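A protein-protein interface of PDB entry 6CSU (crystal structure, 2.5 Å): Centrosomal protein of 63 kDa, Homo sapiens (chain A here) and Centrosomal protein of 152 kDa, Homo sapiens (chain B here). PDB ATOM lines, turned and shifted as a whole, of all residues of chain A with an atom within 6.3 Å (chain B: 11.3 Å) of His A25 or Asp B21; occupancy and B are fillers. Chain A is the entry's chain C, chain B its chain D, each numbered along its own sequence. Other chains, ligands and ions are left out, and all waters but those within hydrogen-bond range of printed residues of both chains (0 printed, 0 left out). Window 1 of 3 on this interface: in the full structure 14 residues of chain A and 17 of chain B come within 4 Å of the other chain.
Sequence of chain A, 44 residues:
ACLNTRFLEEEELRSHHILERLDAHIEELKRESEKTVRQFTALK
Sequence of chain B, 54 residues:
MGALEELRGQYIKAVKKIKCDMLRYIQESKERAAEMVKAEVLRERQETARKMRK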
ATOM      1  N   ILE A  18     -32.147 -10.115 -11.569  1.00  0.00           N
ATOM      2  CA  ILE A  18     -31.201 -11.100 -12.084  1.00  0.00           C
ATOM      3  C   ILE A  18     -31.062 -12.257 -11.104  1.00  0.00           C
ATOM      4  O   ILE A  18     -30.860 -13.409 -11.509  1.00  0.00           O
ATOM      5  CB  ILE A  18     -29.845 -10.423 -12.382  1.00  0.00           C
ATOM      6  CG1 ILE A  18     -28.859 -11.400 -13.016  1.00  0.00           C
ATOM      7  CG2 ILE A  18     -29.240  -9.841 -11.125  1.00  0.00           C
ATOM      8  CD1 ILE A  18     -29.183 -11.736 -14.439  1.00  0.00           C
ATOM      9  N   GLU A  20     -33.536 -13.474  -9.156  1.00  0.00           N
ATOM     10  CA  GLU A  20     -34.689 -14.330  -9.415  1.00  0.00           C
ATOM     11  C   GLU A  20     -34.437 -15.237 -10.607  1.00  0.00           C
ATOM     12  O   GLU A  20     -34.656 -16.452 -10.530  1.00  0.00           O
ATOM     13  CB  GLU A  20     -35.937 -13.482  -9.663  1.00  0.00           C
ATOM     14  CG  GLU A  20     -36.585 -12.911  -8.415  1.00  0.00           C
ATOM     15  CD  GLU A  20     -37.628 -11.854  -8.741  1.00  0.00           C
ATOM     16  OE1 GLU A  20     -38.593 -12.158  -9.474  1.00  0.00           O
ATOM     17  OE2 GLU A  20     -37.473 -10.709  -8.274  1.00  0.00           O
ATOM     18  N   ARG A  21     -33.960 -14.663 -11.713  1.00  0.00           N
ATOM     19  CA  ARG A  21     -33.773 -15.430 -12.937  1.00  0.00           C
ATOM     20  C   ARG A  21     -32.781 -16.565 -12.743  1.00  0.00           C
ATOM     21  O   ARG A  21     -32.911 -17.615 -13.382  1.00  0.00           O
ATOM     22  CB  ARG A  21     -33.319 -14.504 -14.066  1.00  0.00           C
ATOM     23  CG  ARG A  21     -34.385 -14.257 -15.122  1.00  0.00           C
ATOM     24  CD  ARG A  21     -34.149 -12.955 -15.866  1.00  0.00           C
ATOM     25  NE  ARG A  21     -34.374 -11.787 -15.017  1.00  0.00           N
ATOM     26  CZ  ARG A  21     -34.538 -10.550 -15.475  1.00  0.00           C
ATOM     27  NH1 ARG A  21     -34.512 -10.317 -16.781  1.00  0.00           N
ATOM     28  NH2 ARG A  21     -34.737  -9.546 -14.632  1.00  0.00           N
ATOM     29  N   LEU A  22     -31.798 -16.381 -11.860  1.00  0.00           N
ATOM     30  CA  LEU A  22     -30.849 -17.454 -11.585  1.00  0.00           C
ATOM     31  C   LEU A  22     -31.502 -18.558 -10.766  1.00  0.00           C
ATOM     32  O   LEU A  22     -31.328 -19.746 -11.057  1.00  0.00           O
ATOM     33  CB  LEU A  22     -29.619 -16.905 -10.862  1.00  0.00           C
ATOM     34  CG  LEU A  22     -28.731 -15.878 -11.573  1.00  0.00           C
ATOM     35  CD1 LEU A  22     -27.266 -16.132 -11.233  1.00  0.00           C
ATOM     36  CD2 LEU A  22     -28.948 -15.868 -13.082  1.00  0.00           C
ATOM     37  N   ASP A  23     -32.258 -18.179  -9.732  1.00  0.00           N
ATOM     38  CA  ASP A  23     -33.003 -19.167  -8.962  1.00  0.00           C
ATOM     39  C   ASP A  23     -33.966 -19.949  -9.841  1.00  0.00           C
ATOM     40  O   ASP A  23     -34.190 -21.143  -9.608  1.00  0.00           O
ATOM     41  CB  ASP A  23     -33.770 -18.491  -7.826  1.00  0.00           C
ATOM     42  CG  ASP A  23     -32.898 -18.187  -6.630  1.00  0.00           C
ATOM     43  OD1 ASP A  23     -31.715 -18.582  -6.638  1.00  0.00           O
ATOM     44  OD2 ASP A  23     -33.403 -17.565  -5.673  1.00  0.00           O
ATOM     45  N   ALA A  24     -34.546 -19.294 -10.850  1.00  0.00           N
ATOM     46  CA  ALA A  24     -35.470 -19.969 -11.754  1.00  0.00           C
ATOM     47  C   ALA A  24     -34.763 -21.066 -12.538  1.00  0.00           C
ATOM     48  O   ALA A  24     -35.193 -22.225 -12.541  1.00  0.00           O
ATOM     49  CB  ALA A  24     -36.107 -18.951 -12.701  1.00  0.00           C
ATOM     50  N   HIS A  25     -33.668 -20.710 -13.217  1.00  0.00           N
ATOM     51  CA  HIS A  25     -32.925 -21.683 -14.007  1.00  0.00           C
ATOM     52  C   HIS A  25     -32.447 -22.848 -13.153  1.00  0.00           C
ATOM     53  O   HIS A  25     -32.314 -23.973 -13.648  1.00  0.00           O
ATOM     54  CB  HIS A  25     -31.739 -21.002 -14.690  1.00  0.00           C
ATOM     55  CG  HIS A  25     -32.101 -19.757 -15.439  1.00  0.00           C
ATOM     56  ND1 HIS A  25     -33.343 -19.558 -16.005  1.00  0.00           N
ATOM     57  CD2 HIS A  25     -31.382 -18.642 -15.710  1.00  0.00           C
ATOM     58  CE1 HIS A  25     -33.371 -18.377 -16.594  1.00  0.00           C
ATOM     59  NE2 HIS A  25     -32.195 -17.799 -16.430  1.00  0.00           N
ATOM     60  N   ILE A  26     -32.198 -22.604 -11.867  1.00  0.00           N
ATOM     61  CA  ILE A  26     -31.804 -23.677 -10.962  1.00  0.00           C
ATOM     62  C   ILE A  26     -32.998 -24.554 -10.615  1.00  0.00           C
ATOM     63  O   ILE A  26     -32.925 -25.785 -10.698  1.00  0.00           O
ATOM     64  CB  ILE A  26     -31.148 -23.094  -9.698  1.00  0.00           C
ATOM     65  CG1 ILE A  26     -29.827 -22.400 -10.045  1.00  0.00           C
ATOM     66  CG2 ILE A  26     -30.930 -24.181  -8.659  1.00  0.00           C
ATOM     67  CD1 ILE A  26     -29.219 -21.648  -8.874  1.00  0.00           C
ATOM     68  N   GLU A  27     -34.118 -23.933 -10.232  1.00  0.00           N
ATOM     69  CA  GLU A  27     -35.307 -24.695  -9.864  1.00  0.00           C
ATOM     70  C   GLU A  27     -35.820 -25.524 -11.033  1.00  0.00           C
ATOM     71  O   GLU A  27     -36.279 -26.658 -10.851  1.00  0.00           O
ATOM     72  CB  GLU A  27     -36.400 -23.750  -9.363  1.00  0.00           C
ATOM     73  CG  GLU A  27     -37.303 -24.357  -8.307  1.00  0.00           C
ATOM     74  CD  GLU A  27     -36.575 -24.624  -6.994  1.00  0.00           C
ATOM     75  OE1 GLU A  27     -35.599 -23.905  -6.686  1.00  0.00           O
ATOM     76  OE2 GLU A  27     -36.985 -25.553  -6.267  1.00  0.00           O
ATOM     77  N   GLU A  28     -35.754 -24.972 -12.248  1.00  0.00           N
ATOM     78  CA  GLU A  28     -36.127 -25.747 -13.423  1.00  0.00           C
ATOM     79  C   GLU A  28     -35.209 -26.950 -13.594  1.00  0.00           C
ATOM     80  O   GLU A  28     -35.669 -28.045 -13.936  1.00  0.00           O
ATOM     81  CB  GLU A  28     -36.091 -24.869 -14.672  1.00  0.00           C
ATOM     82  CG  GLU A  28     -36.532 -25.593 -15.927  1.00  0.00           C
ATOM     83  CD  GLU A  28     -36.241 -24.812 -17.196  1.00  0.00           C
ATOM     84  OE1 GLU A  28     -35.268 -24.026 -17.211  1.00  0.00           O
ATOM     85  OE2 GLU A  28     -36.988 -24.991 -18.181  1.00  0.00           O
ATOM     86  N   LEU A  29     -33.908 -26.759 -13.355  1.00  0.00           N
ATOM     87  CA  LEU A  29     -32.980 -27.882 -13.427  1.00  0.00           C
ATOM     88  C   LEU A  29     -33.333 -28.941 -12.395  1.00  0.00           C
ATOM     89  O   LEU A  29     -33.287 -30.142 -12.685  1.00  0.00           O
ATOM     90  CB  LEU A  29     -31.545 -27.396 -13.225  1.00  0.00           C
ATOM     91  CG  LEU A  29     -30.464 -28.478 -13.136  1.00  0.00           C
ATOM     92  CD1 LEU A  29     -30.286 -29.156 -14.484  1.00  0.00           C
ATOM     93  CD2 LEU A  29     -29.139 -27.898 -12.643  1.00  0.00           C
ATOM     94  N   LYS A  30     -33.703 -28.512 -11.189  1.00  0.00           N
ATOM     95  CA  LYS A  30     -34.043 -29.470 -10.147  1.00  0.00           C
ATOM     96  C   LYS A  30     -35.278 -30.271 -10.527  1.00  0.00           C
ATOM     97  O   LYS A  30     -35.346 -31.478 -10.273  1.00  0.00           O
ATOM     98  CB  LYS A  30     -34.241 -28.746  -8.814  1.00  0.00           C
ATOM     99  CG  LYS A  30     -33.022 -27.950  -8.366  1.00  0.00           C
ATOM    100  CD  LYS A  30     -32.798 -28.049  -6.867  1.00  0.00           C
ATOM    101  CE  LYS A  30     -33.135 -26.751  -6.154  1.00  0.00           C
ATOM    102  NZ  LYS A  30     -34.336 -26.901  -5.287  1.00  0.00           N
ATOM    103  N   LEU B   7     -29.473 -35.655 -18.377  1.00  0.00           N
ATOM    104  CA  LEU B   7     -28.961 -34.875 -17.258  1.00  0.00           C
ATOM    105  C   LEU B   7     -27.871 -33.919 -17.715  1.00  0.00           C
ATOM    106  O   LEU B   7     -27.829 -32.761 -17.283  1.00  0.00           O
ATOM    107  CB  LEU B   7     -28.432 -35.804 -16.167  1.00  0.00           C
ATOM    108  CG  LEU B   7     -29.461 -36.623 -15.385  1.00  0.00           C
ATOM    109  CD1 LEU B   7     -28.776 -37.447 -14.296  1.00  0.00           C
ATOM    110  CD2 LEU B   7     -30.526 -35.717 -14.792  1.00  0.00           C
ATOM    111  N   GLY B   9     -27.681 -32.690 -20.693  1.00  0.00           N
ATOM    112  CA  GLY B   9     -28.348 -31.660 -21.465  1.00  0.00           C
ATOM    113  C   GLY B   9     -29.011 -30.618 -20.584  1.00  0.00           C
ATOM    114  O   GLY B   9     -29.019 -29.430 -20.909  1.00  0.00           O
ATOM    115  N   GLN B  10     -29.558 -31.056 -19.449  1.00  0.00           N
ATOM    116  CA  GLN B  10     -30.232 -30.130 -18.546  1.00  0.00           C
ATOM    117  C   GLN B  10     -29.235 -29.218 -17.849  1.00  0.00           C
ATOM    118  O   GLN B  10     -29.509 -28.030 -17.649  1.00  0.00           O
ATOM    119  CB  GLN B  10     -31.053 -30.908 -17.520  1.00  0.00           C
ATOM    120  CG  GLN B  10     -32.191 -31.718 -18.108  1.00  0.00           C
ATOM    121  CD  GLN B  10     -32.653 -32.819 -17.177  1.00  0.00           C
ATOM    122  OE1 GLN B  10     -32.038 -33.063 -16.138  1.00  0.00           O
ATOM    123  NE2 GLN B  10     -33.738 -33.494 -17.545  1.00  0.00           N
ATOM    124  N   TYR B  11     -28.078 -29.756 -17.459  1.00  0.00           N
ATOM    125  CA  TYR B  11     -27.043 -28.910 -16.877  1.00  0.00           C
ATOM    126  C   TYR B  11     -26.606 -27.837 -17.865  1.00  0.00           C
ATOM    127  O   TYR B  11     -26.549 -26.649 -17.528  1.00  0.00           O
ATOM    128  CB  TYR B  11     -25.844 -29.752 -16.445  1.00  0.00           C
ATOM    129  CG  TYR B  11     -24.648 -28.908 -16.057  1.00  0.00           C
ATOM    130  CD1 TYR B  11     -23.686 -28.547 -16.995  1.00  0.00           C
ATOM    131  CD2 TYR B  11     -24.486 -28.461 -14.754  1.00  0.00           C
ATOM    132  CE1 TYR B  11     -22.599 -27.770 -16.645  1.00  0.00           C
ATOM    133  CE2 TYR B  11     -23.398 -27.687 -14.394  1.00  0.00           C
ATOM    134  CZ  TYR B  11     -22.460 -27.342 -15.345  1.00  0.00           C
ATOM    135  OH  TYR B  11     -21.376 -26.571 -14.994  1.00  0.00           O
ATOM    136  N   ILE B  12     -26.288 -28.250 -19.096  1.00  0.00           N
ATOM    137  CA  ILE B  12     -25.807 -27.318 -20.112  1.00  0.00           C
ATOM    138  C   ILE B  12     -26.831 -26.221 -20.354  1.00  0.00           C
ATOM    139  O   ILE B  12     -26.486 -25.038 -20.472  1.00  0.00           O
ATOM    140  CB  ILE B  12     -25.475 -28.075 -21.412  1.00  0.00           C
ATOM    141  CG1 ILE B  12     -24.291 -29.022 -21.202  1.00  0.00           C
ATOM    142  CG2 ILE B  12     -25.203 -27.105 -22.555  1.00  0.00           C
ATOM    143  CD1 ILE B  12     -23.002 -28.326 -20.833  1.00  0.00           C
ATOM    144  N   LYS B  13     -28.110 -26.594 -20.424  1.00  0.00           N
ATOM    145  CA  LYS B  13     -29.155 -25.601 -20.646  1.00  0.00           C
ATOM    146  C   LYS B  13     -29.236 -24.619 -19.486  1.00  0.00           C
ATOM    147  O   LYS B  13     -29.397 -23.410 -19.699  1.00  0.00           O
ATOM    148  CB  LYS B  13     -30.504 -26.290 -20.858  1.00  0.00           C
ATOM    149  CG  LYS B  13     -31.676 -25.320 -20.891  1.00  0.00           C
ATOM    150  CD  LYS B  13     -32.980 -25.969 -20.476  1.00  0.00           C
ATOM    151  CE  LYS B  13     -33.516 -26.873 -21.561  1.00  0.00           C
ATOM    152  NZ  LYS B  13     -34.925 -27.265 -21.283  1.00  0.00           N
ATOM    153  N   ALA B  14     -29.121 -25.118 -18.253  1.00  0.00           N
ATOM    154  CA  ALA B  14     -29.177 -24.241 -17.088  1.00  0.00           C
ATOM    155  C   ALA B  14     -28.077 -23.192 -17.142  1.00  0.00           C
ATOM    156  O   ALA B  14     -28.338 -21.998 -16.982  1.00  0.00           O
ATOM    157  CB  ALA B  14     -29.076 -25.059 -15.800  1.00  0.00           C
ATOM    158  N   VAL B  15     -26.837 -23.623 -17.389  1.00  0.00           N
ATOM    159  CA  VAL B  15     -25.713 -22.692 -17.359  1.00  0.00           C
ATOM    160  C   VAL B  15     -25.741 -21.760 -18.566  1.00  0.00           C
ATOM    161  O   VAL B  15     -25.334 -20.597 -18.466  1.00  0.00           O
ATOM    162  CB  VAL B  15     -24.377 -23.457 -17.261  1.00  0.00           C
ATOM    163  CG1 VAL B  15     -24.416 -24.467 -16.124  1.00  0.00           C
ATOM    164  CG2 VAL B  15     -24.045 -24.146 -18.572  1.00  0.00           C
ATOM    165  N   LYS B  16     -26.226 -22.239 -19.717  1.00  0.00           N
ATOM    166  CA  LYS B  16     -26.300 -21.372 -20.888  1.00  0.00           C
ATOM    167  C   LYS B  16     -27.357 -20.293 -20.713  1.00  0.00           C
ATOM    168  O   LYS B  16     -27.264 -19.231 -21.334  1.00  0.00           O
ATOM    169  CB  LYS B  16     -26.573 -22.198 -22.148  1.00  0.00           C
ATOM    170  CG  LYS B  16     -25.313 -22.662 -22.867  1.00  0.00           C
ATOM    171  CD  LYS B  16     -25.611 -23.744 -23.899  1.00  0.00           C
ATOM    172  CE  LYS B  16     -26.490 -23.235 -25.032  1.00  0.00           C
ATOM    173  NZ  LYS B  16     -26.916 -24.345 -25.935  1.00  0.00           N
ATOM    174  N   LYS B  17     -28.365 -20.546 -19.877  1.00  0.00           N
ATOM    175  CA  LYS B  17     -29.328 -19.504 -19.540  1.00  0.00           C
ATOM    176  C   LYS B  17     -28.741 -18.513 -18.547  1.00  0.00           C
ATOM    177  O   LYS B  17     -29.031 -17.315 -18.617  1.00  0.00           O
ATOM    178  CB  LYS B  17     -30.604 -20.119 -18.969  1.00  0.00           C
ATOM    179  CG  LYS B  17     -31.525 -20.703 -20.015  1.00  0.00           C
ATOM    180  CD  LYS B  17     -32.791 -21.255 -19.387  1.00  0.00           C
ATOM    181  CE  LYS B  17     -33.691 -21.866 -20.446  1.00  0.00           C
ATOM    182  NZ  LYS B  17     -34.922 -22.467 -19.866  1.00  0.00           N
ATOM    183  N   ILE B  18     -27.930 -19.001 -17.608  1.00  0.00           N
ATOM    184  CA  ILE B  18     -27.274 -18.113 -16.654  1.00  0.00           C
ATOM    185  C   ILE B  18     -26.326 -17.171 -17.382  1.00  0.00           C
ATOM    186  O   ILE B  18     -26.246 -15.978 -17.069  1.00  0.00           O
ATOM    187  CB  ILE B  18     -26.550 -18.942 -15.576  1.00  0.00           C
ATOM    188  CG1 ILE B  18     -27.568 -19.636 -14.666  1.00  0.00           C
ATOM    189  CG2 ILE B  18     -25.597 -18.080 -14.762  1.00  0.00           C
ATOM    190  CD1 ILE B  18     -26.926 -20.453 -13.576  1.00  0.00           C
ATOM    191  N   LYS B  19     -25.613 -17.688 -18.382  1.00  0.00           N
ATOM    192  CA  LYS B  19     -24.715 -16.851 -19.168  1.00  0.00           C
ATOM    193  C   LYS B  19     -25.491 -15.820 -19.978  1.00  0.00           C
ATOM    194  O   LYS B  19     -25.085 -14.656 -20.061  1.00  0.00           O
ATOM    195  CB  LYS B  19     -23.864 -17.730 -20.082  1.00  0.00           C
ATOM    196  CG  LYS B  19     -23.019 -16.980 -21.088  1.00  0.00           C
ATOM    197  CD  LYS B  19     -22.308 -17.961 -22.011  1.00  0.00           C
ATOM    198  CE  LYS B  19     -21.473 -17.245 -23.057  1.00  0.00           C
ATOM    199  NZ  LYS B  19     -20.771 -18.209 -23.949  1.00  0.00           N
ATOM    200  N   CYS B  20     -26.612 -16.228 -20.579  1.00  0.00           N
ATOM    201  CA  CYS B  20     -27.433 -15.274 -21.319  1.00  0.00           C
ATOM    202  C   CYS B  20     -27.947 -14.171 -20.406  1.00  0.00           C
ATOM    203  O   CYS B  20     -28.004 -13.002 -20.804  1.00  0.00           O
ATOM    204  CB  CYS B  20     -28.599 -15.991 -21.997  1.00  0.00           C
ATOM    205  SG  CYS B  20     -28.128 -16.955 -23.450  1.00  0.00           S
ATOM    206  N   ASP B  21     -28.329 -14.524 -19.177  1.00  0.00           N
ATOM    207  CA  ASP B  21     -28.809 -13.519 -18.237  1.00  0.00           C
ATOM    208  C   ASP B  21     -27.692 -12.566 -17.830  1.00  0.00           C
ATOM    209  O   ASP B  21     -27.900 -11.349 -17.772  1.00  0.00           O
ATOM    210  CB  ASP B  21     -29.421 -14.193 -17.008  1.00  0.00           C
ATOM    211  CG  ASP B  21     -30.825 -14.715 -17.264  1.00  0.00           C
ATOM    212  OD1 ASP B  21     -31.394 -14.401 -18.332  1.00  0.00           O
ATOM    213  OD2 ASP B  21     -31.366 -15.425 -16.390  1.00  0.00           O
ATOM    214  N   MET B  22     -26.496 -13.097 -17.561  1.00  0.00           N
ATOM    215  CA  MET B  22     -25.380 -12.243 -17.165  1.00  0.00           C
ATOM    216  C   MET B  22     -24.912 -11.366 -18.318  1.00  0.00           C
ATOM    217  O   MET B  22     -24.541 -10.205 -18.110  1.00  0.00           O
ATOM    218  CB  MET B  22     -24.225 -13.094 -16.647  1.00  0.00           C
ATOM    219  CG  MET B  22     -24.538 -13.821 -15.363  1.00  0.00           C
ATOM    220  SD  MET B  22     -25.052 -12.713 -14.032  1.00  0.00           S
ATOM    221  CE  MET B  22     -23.600 -11.677 -13.849  1.00  0.00           C
ATOM    222  N   LEU B  23     -24.910 -11.911 -19.538  1.00  0.00           N
ATOM    223  CA  LEU B  23     -24.546 -11.125 -20.712  1.00  0.00           C
ATOM    224  C   LEU B  23     -25.437  -9.898 -20.853  1.00  0.00           C
ATOM    225  O   LEU B  23     -24.958  -8.794 -21.134  1.00  0.00           O
ATOM    226  CB  LEU B  23     -24.635 -11.993 -21.969  1.00  0.00           C
ATOM    227  CG  LEU B  23     -23.472 -12.948 -22.231  1.00  0.00           C
ATOM    228  CD1 LEU B  23     -23.733 -13.826 -23.451  1.00  0.00           C
ATOM    229  CD2 LEU B  23     -22.212 -12.142 -22.413  1.00  0.00           C
ATOM    230  N   ARG B  24     -26.746 -10.079 -20.668  1.00  0.00           N
ATOM    231  CA  ARG B  24     -27.671  -8.958 -20.789  1.00  0.00           C
ATOM    232  C   ARG B  24     -27.573  -8.027 -19.588  1.00  0.00           C
ATOM    233  O   ARG B  24     -27.657  -6.803 -19.736  1.00  0.00           O
ATOM    234  CB  ARG B  24     -29.100  -9.472 -20.951  1.00  0.00           C
ATOM    235  CG  ARG B  24     -29.574  -9.577 -22.394  1.00  0.00           C
ATOM    236  CD  ARG B  24     -29.705  -8.205 -23.055  1.00  0.00           C
ATOM    237  NE  ARG B  24     -28.646  -7.947 -24.031  1.00  0.00           N
ATOM    238  CZ  ARG B  24     -28.630  -6.906 -24.858  1.00  0.00           C
ATOM    239  NH1 ARG B  24     -29.621  -6.025 -24.834  1.00  0.00           N
ATOM    240  NH2 ARG B  24     -27.626  -6.748 -25.710  1.00  0.00           N
ATOM    241  N   TYR B  25     -27.409  -8.590 -18.389  1.00  0.00           N
ATOM    242  CA  TYR B  25     -27.231  -7.765 -17.197  1.00  0.00           C
ATOM    243  C   TYR B  25     -25.999  -6.879 -17.322  1.00  0.00           C
ATOM    244  O   TYR B  25     -26.027  -5.704 -16.942  1.00  0.00           O
ATOM    245  CB  TYR B  25     -27.135  -8.663 -15.961  1.00  0.00           C
ATOM    246  CG  TYR B  25     -26.607  -8.001 -14.701  1.00  0.00           C
ATOM    247  CD1 TYR B  25     -27.452  -7.293 -13.854  1.00  0.00           C
ATOM    248  CD2 TYR B  25     -25.266  -8.116 -14.341  1.00  0.00           C
ATOM    249  CE1 TYR B  25     -26.971  -6.699 -12.692  1.00  0.00           C
ATOM    250  CE2 TYR B  25     -24.777  -7.522 -13.182  1.00  0.00           C
ATOM    251  CZ  TYR B  25     -25.633  -6.817 -12.360  1.00  0.00           C
ATOM    252  OH  TYR B  25     -25.153  -6.227 -11.208  1.00  0.00           O
ATOM    253  N   ILE B  26     -24.914  -7.426 -17.872  1.00  0.00           N
ATOM    254  CA  ILE B  26     -23.669  -6.675 -17.995  1.00  0.00           C
ATOM    255  C   ILE B  26     -23.804  -5.576 -19.044  1.00  0.00           C
ATOM    256  O   ILE B  26     -23.455  -4.415 -18.797  1.00  0.00           O
ATOM    257  CB  ILE B  26     -22.508  -7.630 -18.326  1.00  0.00           C
ATOM    258  CG1 ILE B  26     -22.072  -8.391 -17.071  1.00  0.00           C
ATOM    259  CG2 ILE B  26     -21.346  -6.871 -18.949  1.00  0.00           C
ATOM    260  CD1 ILE B  26     -21.057  -9.474 -17.342  1.00  0.00           C
ATOM    261  N   GLN B  27     -24.294  -5.933 -20.236  1.00  0.00           N
ATOM    262  CA  GLN B  27     -24.503  -4.936 -21.280  1.00  0.00           C
ATOM    263  C   GLN B  27     -25.392  -3.807 -20.780  1.00  0.00           C
ATOM    264  O   GLN B  27     -25.119  -2.630 -21.039  1.00  0.00           O
ATOM    265  CB  GLN B  27     -25.113  -5.594 -22.520  1.00  0.00           C
ATOM    266  CG  GLN B  27     -25.506  -4.616 -23.619  1.00  0.00           C
ATOM    267  CD  GLN B  27     -24.307  -3.936 -24.259  1.00  0.00           C
ATOM    268  OE1 GLN B  27     -23.208  -4.491 -24.290  1.00  0.00           O
ATOM    269  NE2 GLN B  27     -24.515  -2.725 -24.770  1.00  0.00           N
ATOM    270  N   GLU B  28     -26.450  -4.150 -20.043  1.00  0.00           N
ATOM    271  CA  GLU B  28     -27.306  -3.126 -19.454  1.00  0.00           C
ATOM    272  C   GLU B  28     -26.538  -2.284 -18.443  1.00  0.00           C
ATOM    273  O   GLU B  28     -26.694  -1.059 -18.399  1.00  0.00           O
ATOM    274  CB  GLU B  28     -28.524  -3.780 -18.799  1.00  0.00           C
ATOM    275  CG  GLU B  28     -29.495  -2.805 -18.144  1.00  0.00           C
ATOM    276  CD  GLU B  28     -30.208  -1.926 -19.154  1.00  0.00           C
ATOM    277  OE1 GLU B  28     -30.360  -2.360 -20.316  1.00  0.00           O
ATOM    278  OE2 GLU B  28     -30.611  -0.799 -18.789  1.00  0.00           O
ATOM    279  N   SER B  29     -25.689  -2.921 -17.633  1.00  0.00           N
ATOM    280  CA  SER B  29     -24.975  -2.181 -16.598  1.00  0.00           C
ATOM    281  C   SER B  29     -23.984  -1.196 -17.207  1.00  0.00           C
ATOM    282  O   SER B  29     -23.800  -0.091 -16.685  1.00  0.00           O
ATOM    283  CB  SER B  29     -24.262  -3.150 -15.654  1.00  0.00           C
ATOM    284  OG  SER B  29     -23.917  -2.516 -14.431  1.00  0.00           O
ATOM    285  N   LYS B  30     -23.346  -1.572 -18.317  1.00  0.00           N
ATOM    286  CA  LYS B  30     -22.376  -0.679 -18.941  1.00  0.00           C
ATOM    287  C   LYS B  30     -23.064   0.491 -19.634  1.00  0.00           C
ATOM    288  O   LYS B  30     -22.527   1.605 -19.657  1.00  0.00           O
ATOM    289  CB  LYS B  30     -21.502  -1.459 -19.921  1.00  0.00           C
ATOM    290  CG  LYS B  30     -20.481  -2.366 -19.249  1.00  0.00           C
ATOM    291  CD  LYS B  30     -20.185  -3.592 -20.097  1.00  0.00           C
ATOM    292  CE  LYS B  30     -19.852  -3.206 -21.523  1.00  0.00           C
ATOM    293  NZ  LYS B  30     -19.562  -4.399 -22.370  1.00  0.00           N
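Hydrophobic or aromatic side chains of chain A that line the printed part of chain B: Ile A18, His A25 and Leu A29.
Of the 23 printed residues of chain B, 6 touch a printed residue of chain A.
Among the printed residues, 9 pairs touch across the chains.
Among the printed residues, Asp or Glu carboxylates within 4 Å of a Lys or Arg side-chain nitrogen of the other chain: Glu A28 with Lys B17.
Of the printed residues of chain B, Ile A18 touches Asp B21 and Tyr B25.
Arg A21 touches one residue of chain B.
No residue of chain B comes within 4 Å of Leu A22.
No residue of chain B comes within 4 Å of Ala A24.
His A25 touches just these residues of chain B: Lys B17, Ile B18 and Asp B21.
Glu A28 touches just one residue of chain B: Lys B17 (3.1 Å).
Leu A29 touches two residues of chain B.
Printed residues of chain A within 4 Å of Gln B10: Leu A29.
Of the printed residues of chain A, Tyr B11 touches Leu A29.
Of the printed residues of chain A, Ile B18 touches His A25.
Of chain A, only Ile A18, Arg A21 and His A25 come within 4 Å of Asp B21.
The nearest residue of chain A that does not touch Asp B21 is Leu A22 (4.1 Å).
The side-chain amino group (NZ) of Lys B17 lies within salt-bridge range of the side-chain carboxylate (OE1) of Glu A28, 3.1 Å away.
The side-chain carboxylate of Asp B21 sits at hydrogen-bond distance from a ring nitrogen (NE2) of His A25 (2.5 Å).
Among the printed residues, merely in contact across the chains: Ile A18 with Asp B21, Ile A18 with Tyr B25, Arg A21 with Asp B21, His A25 with Lys B17, His A25 with Ile B18, Leu A29 with Gln B10 and Leu A29 with Tyr B11.
NE2 of His A25 lies close to O of Arg A21, 3.1 Å away.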
